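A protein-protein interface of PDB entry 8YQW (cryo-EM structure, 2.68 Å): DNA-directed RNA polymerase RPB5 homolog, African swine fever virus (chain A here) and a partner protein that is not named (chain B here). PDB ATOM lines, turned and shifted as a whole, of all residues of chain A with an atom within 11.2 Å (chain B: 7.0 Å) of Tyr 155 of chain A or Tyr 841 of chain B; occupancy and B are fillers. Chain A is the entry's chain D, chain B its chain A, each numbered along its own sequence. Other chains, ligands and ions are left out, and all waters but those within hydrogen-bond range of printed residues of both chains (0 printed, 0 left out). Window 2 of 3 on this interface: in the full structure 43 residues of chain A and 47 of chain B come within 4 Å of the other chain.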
ATOM      1  N   GLU A 146     -22.947  -1.159 -11.293  1.00  0.00           N
ATOM      2  CA  GLU A 146     -23.524  -2.200 -10.450  1.00  0.00           C
ATOM      3  C   GLU A 146     -22.999  -2.104  -9.022  1.00  0.00           C
ATOM      4  O   GLU A 146     -23.764  -2.224  -8.054  1.00  0.00           O
ATOM      5  CB  GLU A 146     -23.214  -3.564 -11.067  1.00  0.00           C
ATOM      6  CG  GLU A 146     -23.819  -4.763 -10.378  1.00  0.00           C
ATOM      7  CD  GLU A 146     -23.585  -6.041 -11.161  1.00  0.00           C
ATOM      8  OE1 GLU A 146     -22.999  -5.963 -12.261  1.00  0.00           O
ATOM      9  OE2 GLU A 146     -23.985  -7.123 -10.683  1.00  0.00           O
ATOM     10  N   ALA A 147     -21.695  -1.863  -8.873  1.00  0.00           N
ATOM     11  CA  ALA A 147     -21.112  -1.702  -7.546  1.00  0.00           C
ATOM     12  C   ALA A 147     -21.665  -0.470  -6.845  1.00  0.00           C
ATOM     13  O   ALA A 147     -21.909  -0.496  -5.636  1.00  0.00           O
ATOM     14  CB  ALA A 147     -19.591  -1.624  -7.647  1.00  0.00           C
ATOM     15  N   GLN A 148     -21.851   0.626  -7.583  1.00  0.00           N
ATOM     16  CA  GLN A 148     -22.421   1.826  -6.981  1.00  0.00           C
ATOM     17  C   GLN A 148     -23.857   1.594  -6.540  1.00  0.00           C
ATOM     18  O   GLN A 148     -24.270   2.085  -5.485  1.00  0.00           O
ATOM     19  CB  GLN A 148     -22.342   3.003  -7.949  1.00  0.00           C
ATOM     20  CG  GLN A 148     -20.960   3.614  -8.063  1.00  0.00           C
ATOM     21  CD  GLN A 148     -20.412   4.060  -6.721  1.00  0.00           C
ATOM     22  OE1 GLN A 148     -19.402   3.540  -6.246  1.00  0.00           O
ATOM     23  NE2 GLN A 148     -21.086   5.016  -6.096  1.00  0.00           N
ATOM     24  N   GLU A 149     -24.637   0.857  -7.330  1.00  0.00           N
ATOM     25  CA  GLU A 149     -25.995   0.531  -6.908  1.00  0.00           C
ATOM     26  C   GLU A 149     -25.988  -0.304  -5.631  1.00  0.00           C
ATOM     27  O   GLU A 149     -26.766  -0.043  -4.702  1.00  0.00           O
ATOM     28  CB  GLU A 149     -26.734  -0.199  -8.027  1.00  0.00           C
ATOM     29  CG  GLU A 149     -28.175  -0.533  -7.698  1.00  0.00           C
ATOM     30  CD  GLU A 149     -29.026   0.702  -7.469  1.00  0.00           C
ATOM     31  OE1 GLU A 149     -28.745   1.747  -8.094  1.00  0.00           O
ATOM     32  OE2 GLU A 149     -29.973   0.630  -6.659  1.00  0.00           O
ATOM     33  N   PHE A 150     -25.100  -1.297  -5.558  1.00  0.00           N
ATOM     34  CA  PHE A 150     -24.987  -2.107  -4.348  1.00  0.00           C
ATOM     35  C   PHE A 150     -24.612  -1.251  -3.142  1.00  0.00           C
ATOM     36  O   PHE A 150     -25.243  -1.337  -2.080  1.00  0.00           O
ATOM     37  CB  PHE A 150     -23.959  -3.220  -4.569  1.00  0.00           C
ATOM     38  CG  PHE A 150     -23.538  -3.917  -3.311  1.00  0.00           C
ATOM     39  CD1 PHE A 150     -24.362  -4.851  -2.712  1.00  0.00           C
ATOM     40  CD2 PHE A 150     -22.315  -3.642  -2.727  1.00  0.00           C
ATOM     41  CE1 PHE A 150     -23.977  -5.493  -1.557  1.00  0.00           C
ATOM     42  CE2 PHE A 150     -21.926  -4.279  -1.572  1.00  0.00           C
ATOM     43  CZ  PHE A 150     -22.758  -5.207  -0.986  1.00  0.00           C
ATOM     44  N   LEU A 151     -23.595  -0.401  -3.296  1.00  0.00           N
ATOM     45  CA  LEU A 151     -23.133   0.428  -2.188  1.00  0.00           C
ATOM     46  C   LEU A 151     -24.200   1.424  -1.757  1.00  0.00           C
ATOM     47  O   LEU A 151     -24.349   1.705  -0.562  1.00  0.00           O
ATOM     48  CB  LEU A 151     -21.850   1.159  -2.579  1.00  0.00           C
ATOM     49  CG  LEU A 151     -20.599   0.315  -2.811  1.00  0.00           C
ATOM     50  CD1 LEU A 151     -19.520   1.148  -3.465  1.00  0.00           C
ATOM     51  CD2 LEU A 151     -20.099  -0.278  -1.512  1.00  0.00           C
ATOM     52  N   GLY A 152     -24.941   1.983  -2.714  1.00  0.00           N
ATOM     53  CA  GLY A 152     -26.007   2.904  -2.368  1.00  0.00           C
ATOM     54  C   GLY A 152     -27.131   2.228  -1.614  1.00  0.00           C
ATOM     55  O   GLY A 152     -27.685   2.798  -0.672  1.00  0.00           O
ATOM     56  N   ARG A 153     -27.487   1.007  -2.016  1.00  0.00           N
ATOM     57  CA  ARG A 153     -28.480   0.263  -1.251  1.00  0.00           C
ATOM     58  C   ARG A 153     -27.980  -0.026   0.158  1.00  0.00           C
ATOM     59  O   ARG A 153     -28.751   0.037   1.122  1.00  0.00           O
ATOM     60  CB  ARG A 153     -28.842  -1.038  -1.966  1.00  0.00           C
ATOM     61  CG  ARG A 153     -30.093  -1.699  -1.421  1.00  0.00           C
ATOM     62  CD  ARG A 153     -29.755  -2.903  -0.566  1.00  0.00           C
ATOM     63  NE  ARG A 153     -30.933  -3.449   0.095  1.00  0.00           N
ATOM     64  CZ  ARG A 153     -30.892  -4.261   1.142  1.00  0.00           C
ATOM     65  NH1 ARG A 153     -29.745  -4.636   1.680  1.00  0.00           N
ATOM     66  NH2 ARG A 153     -32.032  -4.705   1.663  1.00  0.00           N
ATOM     67  N   GLU A 154     -26.694  -0.335   0.300  1.00  0.00           N
ATOM     68  CA  GLU A 154     -26.130  -0.696   1.594  1.00  0.00           C
ATOM     69  C   GLU A 154     -25.638   0.500   2.402  1.00  0.00           C
ATOM     70  O   GLU A 154     -25.141   0.302   3.515  1.00  0.00           O
ATOM     71  CB  GLU A 154     -24.981  -1.689   1.406  1.00  0.00           C
ATOM     72  CG  GLU A 154     -25.363  -2.929   0.636  1.00  0.00           C
ATOM     73  CD  GLU A 154     -25.885  -4.032   1.526  1.00  0.00           C
ATOM     74  OE1 GLU A 154     -25.241  -4.320   2.554  1.00  0.00           O
ATOM     75  OE2 GLU A 154     -26.940  -4.609   1.197  1.00  0.00           O
ATOM     76  N   TYR A 155     -25.765   1.722   1.880  1.00  0.00           N
ATOM     77  CA  TYR A 155     -25.264   2.929   2.547  1.00  0.00           C
ATOM     78  C   TYR A 155     -23.775   2.811   2.859  1.00  0.00           C
ATOM     79  O   TYR A 155     -23.316   3.189   3.937  1.00  0.00           O
ATOM     80  CB  TYR A 155     -26.058   3.242   3.818  1.00  0.00           C
ATOM     81  CG  TYR A 155     -27.314   4.044   3.584  1.00  0.00           C
ATOM     82  CD1 TYR A 155     -27.247   5.376   3.207  1.00  0.00           C
ATOM     83  CD2 TYR A 155     -28.566   3.474   3.745  1.00  0.00           C
ATOM     84  CE1 TYR A 155     -28.392   6.113   2.992  1.00  0.00           C
ATOM     85  CE2 TYR A 155     -29.714   4.203   3.531  1.00  0.00           C
ATOM     86  CZ  TYR A 155     -29.621   5.522   3.157  1.00  0.00           C
ATOM     87  OH  TYR A 155     -30.764   6.253   2.944  1.00  0.00           O
ATOM     88  N   LEU A 156     -23.013   2.290   1.905  1.00  0.00           N
ATOM     89  CA  LEU A 156     -21.602   2.008   2.102  1.00  0.00           C
ATOM     90  C   LEU A 156     -20.753   2.841   1.153  1.00  0.00           C
ATOM     91  O   LEU A 156     -21.215   3.307   0.108  1.00  0.00           O
ATOM     92  CB  LEU A 156     -21.297   0.520   1.883  1.00  0.00           C
ATOM     93  CG  LEU A 156     -21.656  -0.471   2.989  1.00  0.00           C
ATOM     94  CD1 LEU A 156     -21.466  -1.888   2.491  1.00  0.00           C
ATOM     95  CD2 LEU A 156     -20.822  -0.224   4.230  1.00  0.00           C
ATOM     96  N   GLN A 157     -19.502   3.030   1.541  1.00  0.00           N
ATOM     97  CA  GLN A 157     -18.460   3.574   0.692  1.00  0.00           C
ATOM     98  C   GLN A 157     -17.529   2.456   0.248  1.00  0.00           C
ATOM     99  O   GLN A 157     -17.451   1.407   0.896  1.00  0.00           O
ATOM    100  CB  GLN A 157     -17.658   4.653   1.430  1.00  0.00           C
ATOM    101  CG  GLN A 157     -18.507   5.686   2.147  1.00  0.00           C
ATOM    102  CD  GLN A 157     -19.087   6.720   1.205  1.00  0.00           C
ATOM    103  OE1 GLN A 157     -18.486   7.055   0.184  1.00  0.00           O
ATOM    104  NE2 GLN A 157     -20.262   7.237   1.544  1.00  0.00           N
ATOM    105  N   PRO A 158     -16.814   2.633  -0.864  1.00  0.00           N
ATOM    106  CA  PRO A 158     -15.876   1.586  -1.301  1.00  0.00           C
ATOM    107  C   PRO A 158     -14.791   1.279  -0.286  1.00  0.00           C
ATOM    108  O   PRO A 158     -14.179   0.209  -0.361  1.00  0.00           O
ATOM    109  CB  PRO A 158     -15.286   2.166  -2.591  1.00  0.00           C
ATOM    110  CG  PRO A 158     -16.332   3.092  -3.090  1.00  0.00           C
ATOM    111  CD  PRO A 158     -16.961   3.694  -1.875  1.00  0.00           C
ATOM    112  N   GLN A 159     -14.537   2.179   0.662  1.00  0.00           N
ATOM    113  CA  GLN A 159     -13.496   1.978   1.659  1.00  0.00           C
ATOM    114  C   GLN A 159     -13.966   1.174   2.861  1.00  0.00           C
ATOM    115  O   GLN A 159     -13.153   0.878   3.742  1.00  0.00           O
ATOM    116  CB  GLN A 159     -12.958   3.333   2.124  1.00  0.00           C
ATOM    117  CG  GLN A 159     -12.113   4.054   1.086  1.00  0.00           C
ATOM    118  CD  GLN A 159     -12.938   4.649  -0.041  1.00  0.00           C
ATOM    119  OE1 GLN A 159     -14.054   5.121   0.172  1.00  0.00           O
ATOM    120  NE2 GLN A 159     -12.391   4.625  -1.249  1.00  0.00           N
ATOM    121  N   ASP A 160     -15.247   0.815   2.925  1.00  0.00           N
ATOM    122  CA  ASP A 160     -15.752  -0.030   3.997  1.00  0.00           C
ATOM    123  C   ASP A 160     -15.764  -1.505   3.632  1.00  0.00           C
ATOM    124  O   ASP A 160     -15.812  -2.350   4.531  1.00  0.00           O
ATOM    125  CB  ASP A 160     -17.168   0.396   4.387  1.00  0.00           C
ATOM    126  CG  ASP A 160     -17.288   1.883   4.612  1.00  0.00           C
ATOM    127  OD1 ASP A 160     -16.401   2.460   5.271  1.00  0.00           O
ATOM    128  OD2 ASP A 160     -18.275   2.478   4.135  1.00  0.00           O
ATOM    129  N   LEU A 161     -15.721  -1.830   2.345  1.00  0.00           N
ATOM    130  CA  LEU A 161     -15.752  -3.214   1.906  1.00  0.00           C
ATOM    131  C   LEU A 161     -14.456  -3.926   2.273  1.00  0.00           C
ATOM    132  O   LEU A 161     -13.417  -3.305   2.508  1.00  0.00           O
ATOM    133  CB  LEU A 161     -15.964  -3.292   0.396  1.00  0.00           C
ATOM    134  CG  LEU A 161     -17.227  -2.657  -0.176  1.00  0.00           C
ATOM    135  CD1 LEU A 161     -17.210  -2.747  -1.685  1.00  0.00           C
ATOM    136  CD2 LEU A 161     -18.460  -3.331   0.387  1.00  0.00           C
ATOM    137  N   VAL A 195     -22.056 -14.841  -1.269  1.00  0.00           N
ATOM    138  CA  VAL A 195     -21.546 -13.855  -2.211  1.00  0.00           C
ATOM    139  C   VAL A 195     -20.946 -12.706  -1.419  1.00  0.00           C
ATOM    140  O   VAL A 195     -21.598 -12.159  -0.523  1.00  0.00           O
ATOM    141  CB  VAL A 195     -22.650 -13.345  -3.153  1.00  0.00           C
ATOM    142  CG1 VAL A 195     -22.205 -12.076  -3.845  1.00  0.00           C
ATOM    143  CG2 VAL A 195     -23.000 -14.397  -4.166  1.00  0.00           C
ATOM    144  N   VAL B 838     -22.697  -6.994  14.974  1.00  0.00           N
ATOM    145  CA  VAL B 838     -23.736  -7.089  13.958  1.00  0.00           C
ATOM    146  C   VAL B 838     -24.458  -5.755  13.847  1.00  0.00           C
ATOM    147  O   VAL B 838     -24.960  -5.219  14.841  1.00  0.00           O
ATOM    148  CB  VAL B 838     -24.716  -8.223  14.294  1.00  0.00           C
ATOM    149  CG1 VAL B 838     -25.858  -8.245  13.302  1.00  0.00           C
ATOM    150  CG2 VAL B 838     -24.000  -9.553  14.306  1.00  0.00           C
ATOM    151  N   ASP B 839     -24.505  -5.204  12.638  1.00  0.00           N
ATOM    152  CA  ASP B 839     -25.185  -3.939  12.410  1.00  0.00           C
ATOM    153  C   ASP B 839     -26.626  -4.201  11.969  1.00  0.00           C
ATOM    154  O   ASP B 839     -27.132  -5.321  12.058  1.00  0.00           O
ATOM    155  CB  ASP B 839     -24.404  -3.083  11.413  1.00  0.00           C
ATOM    156  CG  ASP B 839     -24.197  -3.762  10.083  1.00  0.00           C
ATOM    157  OD1 ASP B 839     -24.710  -4.876   9.886  1.00  0.00           O
ATOM    158  OD2 ASP B 839     -23.512  -3.174   9.224  1.00  0.00           O
ATOM    159  N   TYR B 840     -27.306  -3.160  11.493  1.00  0.00           N
ATOM    160  CA  TYR B 840     -28.713  -3.261  11.136  1.00  0.00           C
ATOM    161  C   TYR B 840     -28.953  -3.993   9.826  1.00  0.00           C
ATOM    162  O   TYR B 840     -30.110  -4.239   9.479  1.00  0.00           O
ATOM    163  CB  TYR B 840     -29.337  -1.869  11.061  1.00  0.00           C
ATOM    164  CG  TYR B 840     -29.501  -1.218  12.409  1.00  0.00           C
ATOM    165  CD1 TYR B 840     -30.303  -1.788  13.381  1.00  0.00           C
ATOM    166  CD2 TYR B 840     -28.848  -0.038  12.712  1.00  0.00           C
ATOM    167  CE1 TYR B 840     -30.450  -1.200  14.613  1.00  0.00           C
ATOM    168  CE2 TYR B 840     -28.991   0.555  13.940  1.00  0.00           C
ATOM    169  CZ  TYR B 840     -29.794  -0.030  14.887  1.00  0.00           C
ATOM    170  OH  TYR B 840     -29.938   0.565  16.114  1.00  0.00           O
ATOM    171  N   TYR B 841     -27.902  -4.337   9.091  1.00  0.00           N
ATOM    172  CA  TYR B 841     -28.024  -5.112   7.869  1.00  0.00           C
ATOM    173  C   TYR B 841     -27.691  -6.581   8.077  1.00  0.00           C
ATOM    174  O   TYR B 841     -27.623  -7.331   7.100  1.00  0.00           O
ATOM    175  CB  TYR B 841     -27.121  -4.528   6.784  1.00  0.00           C
ATOM    176  CG  TYR B 841     -27.640  -3.263   6.152  1.00  0.00           C
ATOM    177  CD1 TYR B 841     -27.497  -2.037   6.784  1.00  0.00           C
ATOM    178  CD2 TYR B 841     -28.267  -3.293   4.919  1.00  0.00           C
ATOM    179  CE1 TYR B 841     -27.969  -0.880   6.206  1.00  0.00           C
ATOM    180  CE2 TYR B 841     -28.740  -2.144   4.335  1.00  0.00           C
ATOM    181  CZ  TYR B 841     -28.589  -0.941   4.981  1.00  0.00           C
ATOM    182  OH  TYR B 841     -29.065   0.203   4.388  1.00  0.00           O
ATOM    183  N   ARG B 842     -27.489  -7.003   9.326  1.00  0.00           N
ATOM    184  CA  ARG B 842     -26.946  -8.308   9.697  1.00  0.00           C
ATOM    185  C   ARG B 842     -25.519  -8.509   9.208  1.00  0.00           C
ATOM    186  O   ARG B 842     -25.015  -9.636   9.232  1.00  0.00           O
ATOM    187  CB  ARG B 842     -27.831  -9.464   9.214  1.00  0.00           C
ATOM    188  CG  ARG B 842     -28.815  -9.981  10.242  1.00  0.00           C
ATOM    189  CD  ARG B 842     -29.884  -8.972  10.511  1.00  0.00           C
ATOM    190  NE  ARG B 842     -30.849  -9.424  11.504  1.00  0.00           N
ATOM    191  CZ  ARG B 842     -32.112  -9.721  11.242  1.00  0.00           C
ATOM    192  NH1 ARG B 842     -32.602  -9.639  10.018  1.00  0.00           N
ATOM    193  NH2 ARG B 842     -32.911 -10.083  12.241  1.00  0.00           N
ATOM    194  N   ARG B 843     -24.858  -7.449   8.758  1.00  0.00           N
ATOM    195  CA  ARG B 843     -23.440  -7.513   8.456  1.00  0.00           C
ATOM    196  C   ARG B 843     -22.628  -7.425   9.739  1.00  0.00           C
ATOM    197  O   ARG B 843     -23.106  -6.967  10.777  1.00  0.00           O
ATOM    198  CB  ARG B 843     -23.026  -6.380   7.519  1.00  0.00           C
ATOM    199  CG  ARG B 843     -23.923  -6.169   6.325  1.00  0.00           C
ATOM    200  CD  ARG B 843     -23.447  -4.985   5.509  1.00  0.00           C
ATOM    201  NE  ARG B 843     -23.427  -3.760   6.299  1.00  0.00           N
ATOM    202  CZ  ARG B 843     -23.936  -2.602   5.902  1.00  0.00           C
ATOM    203  NH1 ARG B 843     -24.490  -2.463   4.712  1.00  0.00           N
ATOM    204  NH2 ARG B 843     -23.881  -1.557   6.720  1.00  0.00           N
ATOM    205  N   VAL B 844     -21.381  -7.868   9.657  1.00  0.00           N
ATOM    206  CA  VAL B 844     -20.424  -7.746  10.746  1.00  0.00           C
ATOM    207  C   VAL B 844     -19.361  -6.748  10.314  1.00  0.00           C
ATOM    208  O   VAL B 844     -18.755  -6.903   9.249  1.00  0.00           O
ATOM    209  CB  VAL B 844     -19.807  -9.107  11.105  1.00  0.00           C
ATOM    210  CG1 VAL B 844     -18.926  -8.983  12.319  1.00  0.00           C
ATOM    211  CG2 VAL B 844     -20.904 -10.121  11.344  1.00  0.00           C
ATOM    212  N   GLN B 853     -20.333  -9.897   5.049  1.00  0.00           N
ATOM    213  CA  GLN B 853     -21.506  -9.340   4.387  1.00  0.00           C
ATOM    214  C   GLN B 853     -22.788  -9.808   5.060  1.00  0.00           C
ATOM    215  O   GLN B 853     -23.821  -9.137   4.971  1.00  0.00           O
ATOM    216  CB  GLN B 853     -21.497  -9.729   2.910  1.00  0.00           C
ATOM    217  CG  GLN B 853     -22.608  -9.117   2.092  1.00  0.00           C
ATOM    218  CD  GLN B 853     -22.402  -7.645   1.851  1.00  0.00           C
ATOM    219  OE1 GLN B 853     -23.166  -6.812   2.332  1.00  0.00           O
ATOM    220  NE2 GLN B 853     -21.364  -7.313   1.100  1.00  0.00           N
ATOM    221  N   LEU B 854     -22.737 -10.953   5.729  1.00  0.00           N
ATOM    222  CA  LEU B 854     -23.849 -11.473   6.506  1.00  0.00           C
ATOM    223  C   LEU B 854     -23.256 -12.380   7.567  1.00  0.00           C
ATOM    224  O   LEU B 854     -22.365 -13.177   7.263  1.00  0.00           O
ATOM    225  CB  LEU B 854     -24.835 -12.240   5.623  1.00  0.00           C
ATOM    226  CG  LEU B 854     -26.214 -12.541   6.205  1.00  0.00           C
ATOM    227  CD1 LEU B 854     -27.019 -11.277   6.345  1.00  0.00           C
ATOM    228  CD2 LEU B 854     -26.936 -13.523   5.328  1.00  0.00           C
ATOM    229  N   TYR B 855     -23.729 -12.251   8.802  1.00  0.00           N
ATOM    230  CA  TYR B 855     -23.148 -13.017   9.894  1.00  0.00           C
ATOM    231  C   TYR B 855     -23.322 -14.511   9.660  1.00  0.00           C
ATOM    232  O   TYR B 855     -24.438 -14.994   9.453  1.00  0.00           O
ATOM    233  CB  TYR B 855     -23.783 -12.623  11.221  1.00  0.00           C
ATOM    234  CG  TYR B 855     -23.345 -13.506  12.359  1.00  0.00           C
ATOM    235  CD1 TYR B 855     -22.029 -13.508  12.788  1.00  0.00           C
ATOM    236  CD2 TYR B 855     -24.241 -14.346  12.997  1.00  0.00           C
ATOM    237  CE1 TYR B 855     -21.620 -14.314  13.820  1.00  0.00           C
ATOM    238  CE2 TYR B 855     -23.839 -15.154  14.033  1.00  0.00           C
ATOM    239  CZ  TYR B 855     -22.527 -15.134  14.441  1.00  0.00           C
ATOM    240  OH  TYR B 855     -22.118 -15.937  15.476  1.00  0.00           O
ATOM    241  N   PHE B 975     -35.128 -11.538   5.641  1.00  0.00           N
ATOM    242  CA  PHE B 975     -33.958 -10.765   6.026  1.00  0.00           C
ATOM    243  C   PHE B 975     -34.153  -9.264   5.891  1.00  0.00           C
ATOM    244  O   PHE B 975     -33.232  -8.515   6.225  1.00  0.00           O
ATOM    245  CB  PHE B 975     -32.749 -11.186   5.190  1.00  0.00           C
ATOM    246  CG  PHE B 975     -32.261 -12.569   5.483  1.00  0.00           C
ATOM    247  CD1 PHE B 975     -31.590 -12.843   6.658  1.00  0.00           C
ATOM    248  CD2 PHE B 975     -32.467 -13.593   4.580  1.00  0.00           C
ATOM    249  CE1 PHE B 975     -31.140 -14.110   6.926  1.00  0.00           C
ATOM    250  CE2 PHE B 975     -32.019 -14.861   4.846  1.00  0.00           C
ATOM    251  CZ  PHE B 975     -31.356 -15.121   6.020  1.00  0.00           C
ATOM    252  N   TYR B 990     -26.723 -11.262  -2.390  1.00  0.00           N
ATOM    253  CA  TYR B 990     -26.184 -11.980  -1.242  1.00  0.00           C
ATOM    254  C   TYR B 990     -27.269 -12.433  -0.273  1.00  0.00           C
ATOM    255  O   TYR B 990     -27.012 -13.317   0.549  1.00  0.00           O
ATOM    256  CB  TYR B 990     -25.145 -11.121  -0.517  1.00  0.00           C
ATOM    257  CG  TYR B 990     -25.705 -10.040   0.378  1.00  0.00           C
ATOM    258  CD1 TYR B 990     -26.051  -8.800  -0.134  1.00  0.00           C
ATOM    259  CD2 TYR B 990     -25.861 -10.250   1.739  1.00  0.00           C
ATOM    260  CE1 TYR B 990     -26.552  -7.811   0.681  1.00  0.00           C
ATOM    261  CE2 TYR B 990     -26.363  -9.266   2.558  1.00  0.00           C
ATOM    262  CZ  TYR B 990     -26.705  -8.048   2.024  1.00  0.00           C
ATOM    263  OH  TYR B 990     -27.205  -7.061   2.838  1.00  0.00           O
ATOM    264  N   LEU B 991     -28.466 -11.852  -0.343  1.00  0.00           N
ATOM    265  CA  LEU B 991     -29.580 -12.318   0.473  1.00  0.00           C
ATOM    266  C   LEU B 991     -30.331 -13.470  -0.173  1.00  0.00           C
ATOM    267  O   LEU B 991     -30.943 -14.275   0.534  1.00  0.00           O
ATOM    268  CB  LEU B 991     -30.554 -11.173   0.756  1.00  0.00           C
ATOM    269  CG  LEU B 991     -30.138 -10.145   1.806  1.00  0.00           C
ATOM    270  CD1 LEU B 991     -31.271  -9.177   2.063  1.00  0.00           C
ATOM    271  CD2 LEU B 991     -29.715 -10.832   3.087  1.00  0.00           C
ATOM    272  N   TYR B1037     -29.606  -7.456  16.020  1.00  0.00           N
ATOM    273  CA  TYR B1037     -28.823  -6.260  15.743  1.00  0.00           C
ATOM    274  C   TYR B1037     -27.996  -5.884  16.962  1.00  0.00           C
ATOM    275  O   TYR B1037     -28.499  -5.872  18.089  1.00  0.00           O
ATOM    276  CB  TYR B1037     -29.736  -5.094  15.375  1.00  0.00           C
ATOM    277  CG  TYR B1037     -30.627  -5.305  14.180  1.00  0.00           C
ATOM    278  CD1 TYR B1037     -30.161  -5.937  13.041  1.00  0.00           C
ATOM    279  CD2 TYR B1037     -31.932  -4.847  14.184  1.00  0.00           C
ATOM    280  CE1 TYR B1037     -30.975  -6.112  11.948  1.00  0.00           C
ATOM    281  CE2 TYR B1037     -32.750  -5.022  13.098  1.00  0.00           C
ATOM    282  CZ  TYR B1037     -32.268  -5.655  11.982  1.00  0.00           C
ATOM    283  OH  TYR B1037     -33.084  -5.831  10.893  1.00  0.00           O
ATOM    284  N   TYR B1426     -27.664  -0.734  21.681  1.00  0.00           N
ATOM    285  CA  TYR B1426     -27.380  -0.536  20.265  1.00  0.00           C
ATOM    286  C   TYR B1426     -28.380   0.416  19.623  1.00  0.00           C
ATOM    287  O   TYR B1426     -27.993   1.350  18.912  1.00  0.00           O
ATOM    288  CB  TYR B1426     -27.367  -1.876  19.531  1.00  0.00           C
ATOM    289  CG  TYR B1426     -26.766  -1.771  18.153  1.00  0.00           C
ATOM    290  CD1 TYR B1426     -25.415  -1.524  17.988  1.00  0.00           C
ATOM    291  CD2 TYR B1426     -27.550  -1.900  17.019  1.00  0.00           C
ATOM    292  CE1 TYR B1426     -24.862  -1.417  16.737  1.00  0.00           C
ATOM    293  CE2 TYR B1426     -27.001  -1.794  15.763  1.00  0.00           C
ATOM    294  CZ  TYR B1426     -25.657  -1.552  15.629  1.00  0.00           C
ATOM    295  OH  TYR B1426     -25.097  -1.443  14.382  1.00  0.00           O
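The backbone carbonyl oxygen of Arg 153 of chain A lies within hydrogen-bond range of the side-chain hydroxyl of Tyr 841 of chain B, 3.3 Å away.
The side-chain carboxylate (OE1) of Glu 154 of chain A lies within salt-bridge range of the guanidinium group (NH1) of Arg 843 of chain B (2.9 Å).
The side-chain amide oxygen (OE1) of Gln 853 of chain B lies close to the side-chain carboxylate (OE1) of Glu 154 of chain A, 3.3 Å away.
The side-chain hydroxyl (OH) of Tyr 990 of chain B sits at hydrogen-bond distance from the side-chain carboxylate (OE2) of Glu 154 of chain A (3.0 Å).
The side-chain carboxylate of Asp 839 of chain B lies close to the backbone NH of Tyr 841 of chain B (3.3 Å).
NE of Arg 843 of chain B is in salt-bridge range of OD2 of Asp 839 of chain B (3.0 Å).
N of Leu 156 of chain A is in hydrogen-bond range of O of Leu 151 of chain A (2.9 Å).
The guanidinium group (NH1) of Arg 153 of chain A lies within salt-bridge range of the side-chain carboxylate (OE2) of Glu 154 of chain A (2.8 Å).
Among the printed residues, pairs that only touch across the chains: Phe 150 of chain A with Gln 853 of chain B, Tyr 155 of chain A with Tyr 841 of chain B, Val 195 of chain A with Tyr 990 of chain B, Arg 153 of chain A with Tyr 990 of chain B, Leu 156 of chain A with Arg 843 of chain B and Glu 154 of chain A with Tyr 841 of chain B.
Printed residues of chain B within 4 Å of Phe 150 of chain A: Gln 853.
Of the printed residues of chain B, Glu 154 of chain A touches Tyr 841 (3.9 Å), Arg 843 (2.9 Å), Gln 853 (3.3 Å) and Tyr 990 (3.0 Å).
Printed residues of chain B within 4 Å of Leu 156 of chain A: Arg 843.
Gln 157 of chain A touches none of the printed residues of chain B.
Of the printed residues of chain A, Tyr 841 of chain B touches Arg 153 (3.3 Å), Glu 154 (3.9 Å) and Tyr 155 (3.4 Å).
Arg 843 of chain B touches just these residues of chain A: Glu 154 and Leu 156.
Printed residues of chain A within 4 Å of Gln 853 of chain B: Phe 150 (3.3 Å) and Glu 154 (3.3 Å).
Of the printed residues of chain A, Tyr 990 of chain B touches Arg 153 (3.7 Å), Glu 154 (3.0 Å) and Val 195 (3.7 Å).
The nearest residue of chain B that does not touch Tyr 155 of chain A is Arg 843 of chain B (5.2 Å).
The nearest residue of chain A that does not touch Tyr 841 of chain B is Gly 152 of chain A (5.9 Å).
Of the 15 printed residues of chain B, 4 touch a printed residue of chain A.
Of the 17 printed residues of chain A, 6 touch a printed residue of chain B.
Hydrophobic or aromatic side chains of chain A within 4 Å of the printed part of chain B: Phe 150, Tyr 155 and Leu 156.
Along chain A the printed residues that touch a printed residue of chain B span positions 150 to 195.
Among the printed residues, 10 pairs touch across the chains.
Among the printed residues, Asp or Glu carboxylates within 4 Å of a Lys or Arg side-chain nitrogen of the other chain: Glu 154 of chain A with Arg 843 of chain B (2.9 Å).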
